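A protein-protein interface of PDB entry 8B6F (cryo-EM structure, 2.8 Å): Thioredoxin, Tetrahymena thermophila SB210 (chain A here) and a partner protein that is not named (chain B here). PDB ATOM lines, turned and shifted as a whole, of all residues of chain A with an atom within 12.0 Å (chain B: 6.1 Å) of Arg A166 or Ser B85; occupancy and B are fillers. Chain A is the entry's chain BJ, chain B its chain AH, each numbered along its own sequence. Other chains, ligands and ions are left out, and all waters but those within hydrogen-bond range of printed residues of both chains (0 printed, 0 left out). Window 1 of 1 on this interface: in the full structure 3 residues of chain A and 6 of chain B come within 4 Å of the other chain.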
ATOM      1  N   HIS A 154     -12.390 -30.144 -10.289  1.00  0.00           N
ATOM      2  CA  HIS A 154     -12.781 -30.455 -11.660  1.00  0.00           C
ATOM      3  C   HIS A 154     -13.259 -29.203 -12.382  1.00  0.00           C
ATOM      4  O   HIS A 154     -12.783 -28.883 -13.476  1.00  0.00           O
ATOM      5  CB  HIS A 154     -13.870 -31.529 -11.652  1.00  0.00           C
ATOM      6  CG  HIS A 154     -14.304 -31.968 -13.016  1.00  0.00           C
ATOM      7  ND1 HIS A 154     -15.153 -31.220 -13.803  1.00  0.00           N
ATOM      8  CD2 HIS A 154     -14.020 -33.085 -13.726  1.00  0.00           C
ATOM      9  CE1 HIS A 154     -15.365 -31.854 -14.942  1.00  0.00           C
ATOM     10  NE2 HIS A 154     -14.691 -32.988 -14.920  1.00  0.00           N
ATOM     11  N   LEU A 157     -10.189 -26.891 -13.131  1.00  0.00           N
ATOM     12  CA  LEU A 157      -9.156 -27.299 -14.077  1.00  0.00           C
ATOM     13  C   LEU A 157      -9.705 -28.122 -15.234  1.00  0.00           C
ATOM     14  O   LEU A 157      -9.523 -27.752 -16.396  1.00  0.00           O
ATOM     15  CB  LEU A 157      -8.066 -28.096 -13.348  1.00  0.00           C
ATOM     16  CG  LEU A 157      -7.342 -27.387 -12.205  1.00  0.00           C
ATOM     17  CD1 LEU A 157      -6.403 -28.354 -11.512  1.00  0.00           C
ATOM     18  CD2 LEU A 157      -6.586 -26.168 -12.707  1.00  0.00           C
ATOM     19  N   ASP A 158     -10.384 -29.232 -14.946  1.00  0.00           N
ATOM     20  CA  ASP A 158     -10.750 -30.163 -16.008  1.00  0.00           C
ATOM     21  C   ASP A 158     -11.808 -29.572 -16.925  1.00  0.00           C
ATOM     22  O   ASP A 158     -11.780 -29.798 -18.140  1.00  0.00           O
ATOM     23  CB  ASP A 158     -11.244 -31.477 -15.406  1.00  0.00           C
ATOM     24  CG  ASP A 158     -10.255 -32.080 -14.438  1.00  0.00           C
ATOM     25  OD1 ASP A 158      -9.893 -31.396 -13.459  1.00  0.00           O
ATOM     26  OD2 ASP A 158      -9.842 -33.239 -14.650  1.00  0.00           O
ATOM     27  N   LYS A 159     -12.752 -28.813 -16.368  1.00  0.00           N
ATOM     28  CA  LYS A 159     -13.782 -28.209 -17.204  1.00  0.00           C
ATOM     29  C   LYS A 159     -13.175 -27.239 -18.206  1.00  0.00           C
ATOM     30  O   LYS A 159     -13.540 -27.249 -19.386  1.00  0.00           O
ATOM     31  CB  LYS A 159     -14.828 -27.510 -16.336  1.00  0.00           C
ATOM     32  CG  LYS A 159     -16.099 -27.162 -17.097  1.00  0.00           C
ATOM     33  CD  LYS A 159     -17.118 -26.449 -16.227  1.00  0.00           C
ATOM     34  CE  LYS A 159     -16.689 -25.026 -15.923  1.00  0.00           C
ATOM     35  NZ  LYS A 159     -17.748 -24.271 -15.196  1.00  0.00           N
ATOM     36  N   GLU A 160     -12.243 -26.399 -17.760  1.00  0.00           N
ATOM     37  CA  GLU A 160     -11.584 -25.485 -18.685  1.00  0.00           C
ATOM     38  C   GLU A 160     -10.754 -26.245 -19.714  1.00  0.00           C
ATOM     39  O   GLU A 160     -10.734 -25.877 -20.893  1.00  0.00           O
ATOM     40  CB  GLU A 160     -10.719 -24.497 -17.907  1.00  0.00           C
ATOM     41  CG  GLU A 160     -11.535 -23.527 -17.068  1.00  0.00           C
ATOM     42  CD  GLU A 160     -10.675 -22.518 -16.337  1.00  0.00           C
ATOM     43  OE1 GLU A 160      -9.472 -22.791 -16.145  1.00  0.00           O
ATOM     44  OE2 GLU A 160     -11.200 -21.450 -15.960  1.00  0.00           O
ATOM     45  N   ILE A 161     -10.057 -27.301 -19.289  1.00  0.00           N
ATOM     46  CA  ILE A 161      -9.260 -28.082 -20.231  1.00  0.00           C
ATOM     47  C   ILE A 161     -10.153 -28.690 -21.304  1.00  0.00           C
ATOM     48  O   ILE A 161      -9.817 -28.679 -22.494  1.00  0.00           O
ATOM     49  CB  ILE A 161      -8.448 -29.159 -19.487  1.00  0.00           C
ATOM     50  CG1 ILE A 161      -7.337 -28.501 -18.664  1.00  0.00           C
ATOM     51  CG2 ILE A 161      -7.854 -30.163 -20.470  1.00  0.00           C
ATOM     52  CD1 ILE A 161      -6.607 -29.449 -17.737  1.00  0.00           C
ATOM     53  N   ASN A 162     -11.304 -29.233 -20.904  1.00  0.00           N
ATOM     54  CA  ASN A 162     -12.232 -29.793 -21.880  1.00  0.00           C
ATOM     55  C   ASN A 162     -12.793 -28.714 -22.793  1.00  0.00           C
ATOM     56  O   ASN A 162     -12.912 -28.920 -24.006  1.00  0.00           O
ATOM     57  CB  ASN A 162     -13.367 -30.528 -21.168  1.00  0.00           C
ATOM     58  CG  ASN A 162     -14.398 -31.074 -22.134  1.00  0.00           C
ATOM     59  OD1 ASN A 162     -14.237 -32.163 -22.681  1.00  0.00           O
ATOM     60  ND2 ASN A 162     -15.464 -30.315 -22.353  1.00  0.00           N
ATOM     61  N   GLU A 163     -13.152 -27.560 -22.231  1.00  0.00           N
ATOM     62  CA  GLU A 163     -13.696 -26.483 -23.049  1.00  0.00           C
ATOM     63  C   GLU A 163     -12.673 -25.963 -24.047  1.00  0.00           C
ATOM     64  O   GLU A 163     -13.049 -25.426 -25.094  1.00  0.00           O
ATOM     65  CB  GLU A 163     -14.192 -25.348 -22.153  1.00  0.00           C
ATOM     66  CG  GLU A 163     -15.431 -25.717 -21.356  1.00  0.00           C
ATOM     67  CD  GLU A 163     -15.823 -24.661 -20.344  1.00  0.00           C
ATOM     68  OE1 GLU A 163     -15.010 -23.754 -20.080  1.00  0.00           O
ATOM     69  OE2 GLU A 163     -16.948 -24.743 -19.809  1.00  0.00           O
ATOM     70  N   TRP A 164     -11.382 -26.102 -23.744  1.00  0.00           N
ATOM     71  CA  TRP A 164     -10.354 -25.711 -24.702  1.00  0.00           C
ATOM     72  C   TRP A 164     -10.137 -26.790 -25.757  1.00  0.00           C
ATOM     73  O   TRP A 164     -10.125 -26.500 -26.958  1.00  0.00           O
ATOM     74  CB  TRP A 164      -9.043 -25.409 -23.981  1.00  0.00           C
ATOM     75  CG  TRP A 164      -7.904 -25.225 -24.925  1.00  0.00           C
ATOM     76  CD1 TRP A 164      -6.786 -25.996 -25.026  1.00  0.00           C
ATOM     77  CD2 TRP A 164      -7.779 -24.201 -25.919  1.00  0.00           C
ATOM     78  NE1 TRP A 164      -5.967 -25.511 -26.017  1.00  0.00           N
ATOM     79  CE2 TRP A 164      -6.556 -24.409 -26.579  1.00  0.00           C
ATOM     80  CE3 TRP A 164      -8.584 -23.126 -26.308  1.00  0.00           C
ATOM     81  CZ2 TRP A 164      -6.116 -23.582 -27.609  1.00  0.00           C
ATOM     82  CZ3 TRP A 164      -8.147 -22.307 -27.330  1.00  0.00           C
ATOM     83  CH2 TRP A 164      -6.923 -22.538 -27.969  1.00  0.00           C
ATOM     84  N   ALA A 165      -9.962 -28.035 -25.327  1.00  0.00           N
ATOM     85  CA  ALA A 165      -9.715 -29.157 -26.223  1.00  0.00           C
ATOM     86  C   ALA A 165     -10.912 -30.093 -26.182  1.00  0.00           C
ATOM     87  O   ALA A 165     -11.244 -30.634 -25.122  1.00  0.00           O
ATOM     88  CB  ALA A 165      -8.441 -29.901 -25.822  1.00  0.00           C
ATOM     89  N   ARG A 166     -11.546 -30.290 -27.333  1.00  0.00           N
ATOM     90  CA  ARG A 166     -12.714 -31.155 -27.433  1.00  0.00           C
ATOM     91  C   ARG A 166     -13.769 -30.772 -26.402  1.00  0.00           C
ATOM     92  O   ARG A 166     -14.370 -29.702 -26.486  1.00  0.00           O
ATOM     93  CB  ARG A 166     -12.312 -32.621 -27.259  1.00  0.00           C
ATOM     94  CG  ARG A 166     -13.492 -33.576 -27.190  1.00  0.00           C
ATOM     95  CD  ARG A 166     -13.067 -35.016 -27.428  1.00  0.00           C
ATOM     96  NE  ARG A 166     -12.044 -35.459 -26.487  1.00  0.00           N
ATOM     97  CZ  ARG A 166     -10.737 -35.406 -26.706  1.00  0.00           C
ATOM     98  NH1 ARG A 166     -10.240 -34.920 -27.832  1.00  0.00           N
ATOM     99  NH2 ARG A 166      -9.906 -35.856 -25.771  1.00  0.00           N
ATOM    100  N   VAL B  81     -18.707 -32.101 -37.491  1.00  0.00           N
ATOM    101  CA  VAL B  81     -17.505 -31.634 -36.806  1.00  0.00           C
ATOM    102  C   VAL B  81     -16.771 -32.839 -36.230  1.00  0.00           C
ATOM    103  O   VAL B  81     -17.404 -33.700 -35.602  1.00  0.00           O
ATOM    104  CB  VAL B  81     -17.850 -30.622 -35.703  1.00  0.00           C
ATOM    105  CG1 VAL B  81     -16.585 -30.100 -35.038  1.00  0.00           C
ATOM    106  CG2 VAL B  81     -18.677 -29.479 -36.269  1.00  0.00           C
ATOM    107  N   PRO B  82     -15.454 -32.954 -36.410  1.00  0.00           N
ATOM    108  CA  PRO B  82     -14.734 -34.086 -35.816  1.00  0.00           C
ATOM    109  C   PRO B  82     -14.902 -34.119 -34.305  1.00  0.00           C
ATOM    110  O   PRO B  82     -14.939 -33.081 -33.641  1.00  0.00           O
ATOM    111  CB  PRO B  82     -13.276 -33.831 -36.216  1.00  0.00           C
ATOM    112  CG  PRO B  82     -13.355 -32.978 -37.419  1.00  0.00           C
ATOM    113  CD  PRO B  82     -14.566 -32.116 -37.234  1.00  0.00           C
ATOM    114  N   GLU B  83     -15.001 -35.334 -33.762  1.00  0.00           N
ATOM    115  CA  GLU B  83     -15.193 -35.485 -32.324  1.00  0.00           C
ATOM    116  C   GLU B  83     -14.023 -34.896 -31.548  1.00  0.00           C
ATOM    117  O   GLU B  83     -14.220 -34.224 -30.529  1.00  0.00           O
ATOM    118  CB  GLU B  83     -15.375 -36.961 -31.973  1.00  0.00           C
ATOM    119  CG  GLU B  83     -16.637 -37.582 -32.545  1.00  0.00           C
ATOM    120  CD  GLU B  83     -17.900 -37.053 -31.894  1.00  0.00           C
ATOM    121  OE1 GLU B  83     -17.793 -36.234 -30.958  1.00  0.00           O
ATOM    122  OE2 GLU B  83     -19.002 -37.460 -32.316  1.00  0.00           O
ATOM    123  N   GLY B  84     -12.797 -35.138 -32.010  1.00  0.00           N
ATOM    124  CA  GLY B  84     -11.627 -34.614 -31.331  1.00  0.00           C
ATOM    125  C   GLY B  84     -11.476 -33.113 -31.439  1.00  0.00           C
ATOM    126  O   GLY B  84     -10.796 -32.508 -30.604  1.00  0.00           O
ATOM    127  N   SER B  85     -12.089 -32.498 -32.445  1.00  0.00           N
ATOM    128  CA  SER B  85     -11.978 -31.064 -32.639  1.00  0.00           C
ATOM    129  C   SER B  85     -12.858 -30.314 -31.643  1.00  0.00           C
ATOM    130  O   SER B  85     -13.783 -30.869 -31.045  1.00  0.00           O
ATOM    131  CB  SER B  85     -12.369 -30.686 -34.067  1.00  0.00           C
ATOM    132  OG  SER B  85     -12.248 -29.290 -34.276  1.00  0.00           O
ATOM    133  N   ASN B  86     -12.553 -29.031 -31.469  1.00  0.00           N
ATOM    134  CA  ASN B  86     -13.316 -28.175 -30.570  1.00  0.00           C
ATOM    135  C   ASN B  86     -14.584 -27.710 -31.274  1.00  0.00           C
ATOM    136  O   ASN B  86     -14.517 -26.980 -32.269  1.00  0.00           O
ATOM    137  CB  ASN B  86     -12.471 -26.984 -30.128  1.00  0.00           C
ATOM    138  CG  ASN B  86     -13.128 -26.178 -29.030  1.00  0.00           C
ATOM    139  OD1 ASN B  86     -14.332 -25.937 -29.054  1.00  0.00           O
ATOM    140  ND2 ASN B  86     -12.335 -25.758 -28.053  1.00  0.00           N
ATOM    141  N   LYS B  87     -15.740 -28.130 -30.755  1.00  0.00           N
ATOM    142  CA  LYS B  87     -16.999 -27.852 -31.438  1.00  0.00           C
ATOM    143  C   LYS B  87     -17.244 -26.355 -31.564  1.00  0.00           C
ATOM    144  O   LYS B  87     -17.678 -25.877 -32.618  1.00  0.00           O
ATOM    145  CB  LYS B  87     -18.155 -28.517 -30.690  1.00  0.00           C
ATOM    146  CG  LYS B  87     -17.969 -30.005 -30.434  1.00  0.00           C
ATOM    147  CD  LYS B  87     -17.875 -30.795 -31.728  1.00  0.00           C
ATOM    148  CE  LYS B  87     -17.743 -32.285 -31.447  1.00  0.00           C
ATOM    149  NZ  LYS B  87     -17.740 -33.090 -32.702  1.00  0.00           N
ATOM    150  N   PHE B  90     -14.574 -24.647 -34.013  1.00  0.00           N
ATOM    151  CA  PHE B  90     -14.684 -25.161 -35.373  1.00  0.00           C
ATOM    152  C   PHE B  90     -15.731 -24.402 -36.179  1.00  0.00           C
ATOM    153  O   PHE B  90     -15.595 -24.268 -37.400  1.00  0.00           O
ATOM    154  CB  PHE B  90     -15.021 -26.651 -35.330  1.00  0.00           C
ATOM    155  CG  PHE B  90     -14.948 -27.333 -36.663  1.00  0.00           C
ATOM    156  CD1 PHE B  90     -16.049 -27.366 -37.501  1.00  0.00           C
ATOM    157  CD2 PHE B  90     -13.782 -27.958 -37.072  1.00  0.00           C
ATOM    158  CE1 PHE B  90     -15.986 -28.001 -38.725  1.00  0.00           C
ATOM    159  CE2 PHE B  90     -13.712 -28.594 -38.294  1.00  0.00           C
ATOM    160  CZ  PHE B  90     -14.815 -28.616 -39.121  1.00  0.00           C
ATOM    161  N   PHE B 143      -7.430 -25.171 -35.278  1.00  0.00           N
ATOM    162  CA  PHE B 143      -8.532 -25.872 -34.629  1.00  0.00           C
ATOM    163  C   PHE B 143      -9.015 -27.084 -35.413  1.00  0.00           C
ATOM    164  O   PHE B 143      -9.627 -27.979 -34.821  1.00  0.00           O
ATOM    165  CB  PHE B 143      -9.693 -24.906 -34.385  1.00  0.00           C
ATOM    166  CG  PHE B 143      -9.415 -23.904 -33.304  1.00  0.00           C
ATOM    167  CD1 PHE B 143      -9.269 -24.316 -31.990  1.00  0.00           C
ATOM    168  CD2 PHE B 143      -9.294 -22.557 -33.597  1.00  0.00           C
ATOM    169  CE1 PHE B 143      -9.010 -23.405 -30.989  1.00  0.00           C
ATOM    170  CE2 PHE B 143      -9.035 -21.638 -32.599  1.00  0.00           C
ATOM    171  CZ  PHE B 143      -8.892 -22.064 -31.292  1.00  0.00           C
ATOM    172  N   SER B 144      -8.761 -27.141 -36.716  1.00  0.00           N
ATOM    173  CA  SER B 144      -8.875 -28.386 -37.465  1.00  0.00           C
ATOM    174  C   SER B 144      -7.532 -29.093 -37.336  1.00  0.00           C
ATOM    175  O   SER B 144      -6.547 -28.686 -37.960  1.00  0.00           O
ATOM    176  CB  SER B 144      -9.234 -28.123 -38.925  1.00  0.00           C
ATOM    177  OG  SER B 144      -8.228 -27.361 -39.570  1.00  0.00           O
ATOM    178  N   LYS B 145      -7.490 -30.146 -36.535  1.00  0.00           N
ATOM    179  CA  LYS B 145      -6.213 -30.720 -36.117  1.00  0.00           C
ATOM    180  C   LYS B 145      -5.491 -31.448 -37.219  1.00  0.00           C
ATOM    181  O   LYS B 145      -4.488 -32.105 -36.917  1.00  0.00           O
ATOM    182  CB  LYS B 145      -6.434 -31.662 -34.933  1.00  0.00           C
ATOM    183  CG  LYS B 145      -6.940 -30.965 -33.678  1.00  0.00           C
ATOM    184  CD  LYS B 145      -5.917 -29.975 -33.136  1.00  0.00           C
ATOM    185  CE  LYS B 145      -6.421 -29.291 -31.880  1.00  0.00           C
ATOM    186  NZ  LYS B 145      -5.460 -28.263 -31.393  1.00  0.00           N
ATOM    187  N   GLU B 235     -10.451 -30.056 -43.709  1.00  0.00           N
ATOM    188  CA  GLU B 235     -11.484 -30.708 -42.911  1.00  0.00           C
ATOM    189  C   GLU B 235     -12.785 -29.919 -42.876  1.00  0.00           C
ATOM    190  O   GLU B 235     -13.644 -30.203 -42.034  1.00  0.00           O
ATOM    191  CB  GLU B 235     -10.984 -30.945 -41.483  1.00  0.00           C
ATOM    192  CG  GLU B 235      -9.967 -32.068 -41.376  1.00  0.00           C
ATOM    193  CD  GLU B 235      -9.453 -32.259 -39.968  1.00  0.00           C
ATOM    194  OE1 GLU B 235      -9.724 -31.389 -39.115  1.00  0.00           O
ATOM    195  OE2 GLU B 235      -8.776 -33.276 -39.715  1.00  0.00           O
ATOM    196  N   TYR B 236     -12.957 -28.946 -43.764  1.00  0.00           N
ATOM    197  CA  TYR B 236     -14.164 -28.135 -43.826  1.00  0.00           C
ATOM    198  C   TYR B 236     -14.878 -28.403 -45.142  1.00  0.00           C
ATOM    199  O   TYR B 236     -14.251 -28.405 -46.206  1.00  0.00           O
ATOM    200  CB  TYR B 236     -13.836 -26.646 -43.698  1.00  0.00           C
ATOM    201  CG  TYR B 236     -13.494 -26.211 -42.293  1.00  0.00           C
ATOM    202  CD1 TYR B 236     -12.219 -26.394 -41.779  1.00  0.00           C
ATOM    203  CD2 TYR B 236     -14.447 -25.610 -41.484  1.00  0.00           C
ATOM    204  CE1 TYR B 236     -11.905 -25.996 -40.496  1.00  0.00           C
ATOM    205  CE2 TYR B 236     -14.143 -25.207 -40.202  1.00  0.00           C
ATOM    206  CZ  TYR B 236     -12.871 -25.402 -39.713  1.00  0.00           C
ATOM    207  OH  TYR B 236     -12.567 -25.002 -38.434  1.00  0.00           O
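ND2 of Asn B86 sits at hydrogen-bond distance from O of Glu A163 (3.1 Å).
The side-chain amide nitrogen (ND2) of Asn B86 lies within hydrogen-bond range of the backbone carbonyl oxygen (O) of Trp A164 (2.6 Å).
The side-chain amino group (NZ) of Lys B87 lies within salt-bridge range of the side-chain carboxylate (OE1) of Glu B83 (3.6 Å).
The side-chain hydroxyl (OG) of Ser B85 lies within hydrogen-bond range of the backbone carbonyl oxygen (O) of Phe B143.
Trp A164 touches Phe B143 (CH2 to CE1, 3.8 Å).
O of Glu B83 touches CD of Arg A166, at 3.4 Å.
Gly B84 touches Arg A166 (O to CB, 3.7 Å).
Ser B85 touches Arg A166.
Ile A161 touches none of the printed residues of chain B.
Of the printed residues of chain B, Glu A163 touches Asn B86.
Of the printed residues of chain B, Trp A164 touches Asn B86 (2.6 Å) and Phe B143 (3.8 Å).
Arg A166 touches three residues of chain B.
No residue of chain A comes within 4 Å of Pro B82.
Of the printed residues of chain A, Glu B83 touches Arg A166.
Printed residues of chain A within 4 Å of Ser B85: Arg A166.
Asn B86 touches just these residues of chain A: Glu A163 and Trp A164.
No residue of chain A comes within 4 Å of Lys B87.
Of the printed residues of chain A, Phe B143 touches Trp A164 (3.8 Å).
No residue of chain A comes within 4 Å of Ser B144.
Lys B145 touches none of the printed residues of chain A.
The nearest residue of chain B that does not touch Arg A166 is Asn B86 (4.3 Å).
Hydrophobic or aromatic side chains of chain B that line the printed part of chain A: Phe B143.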
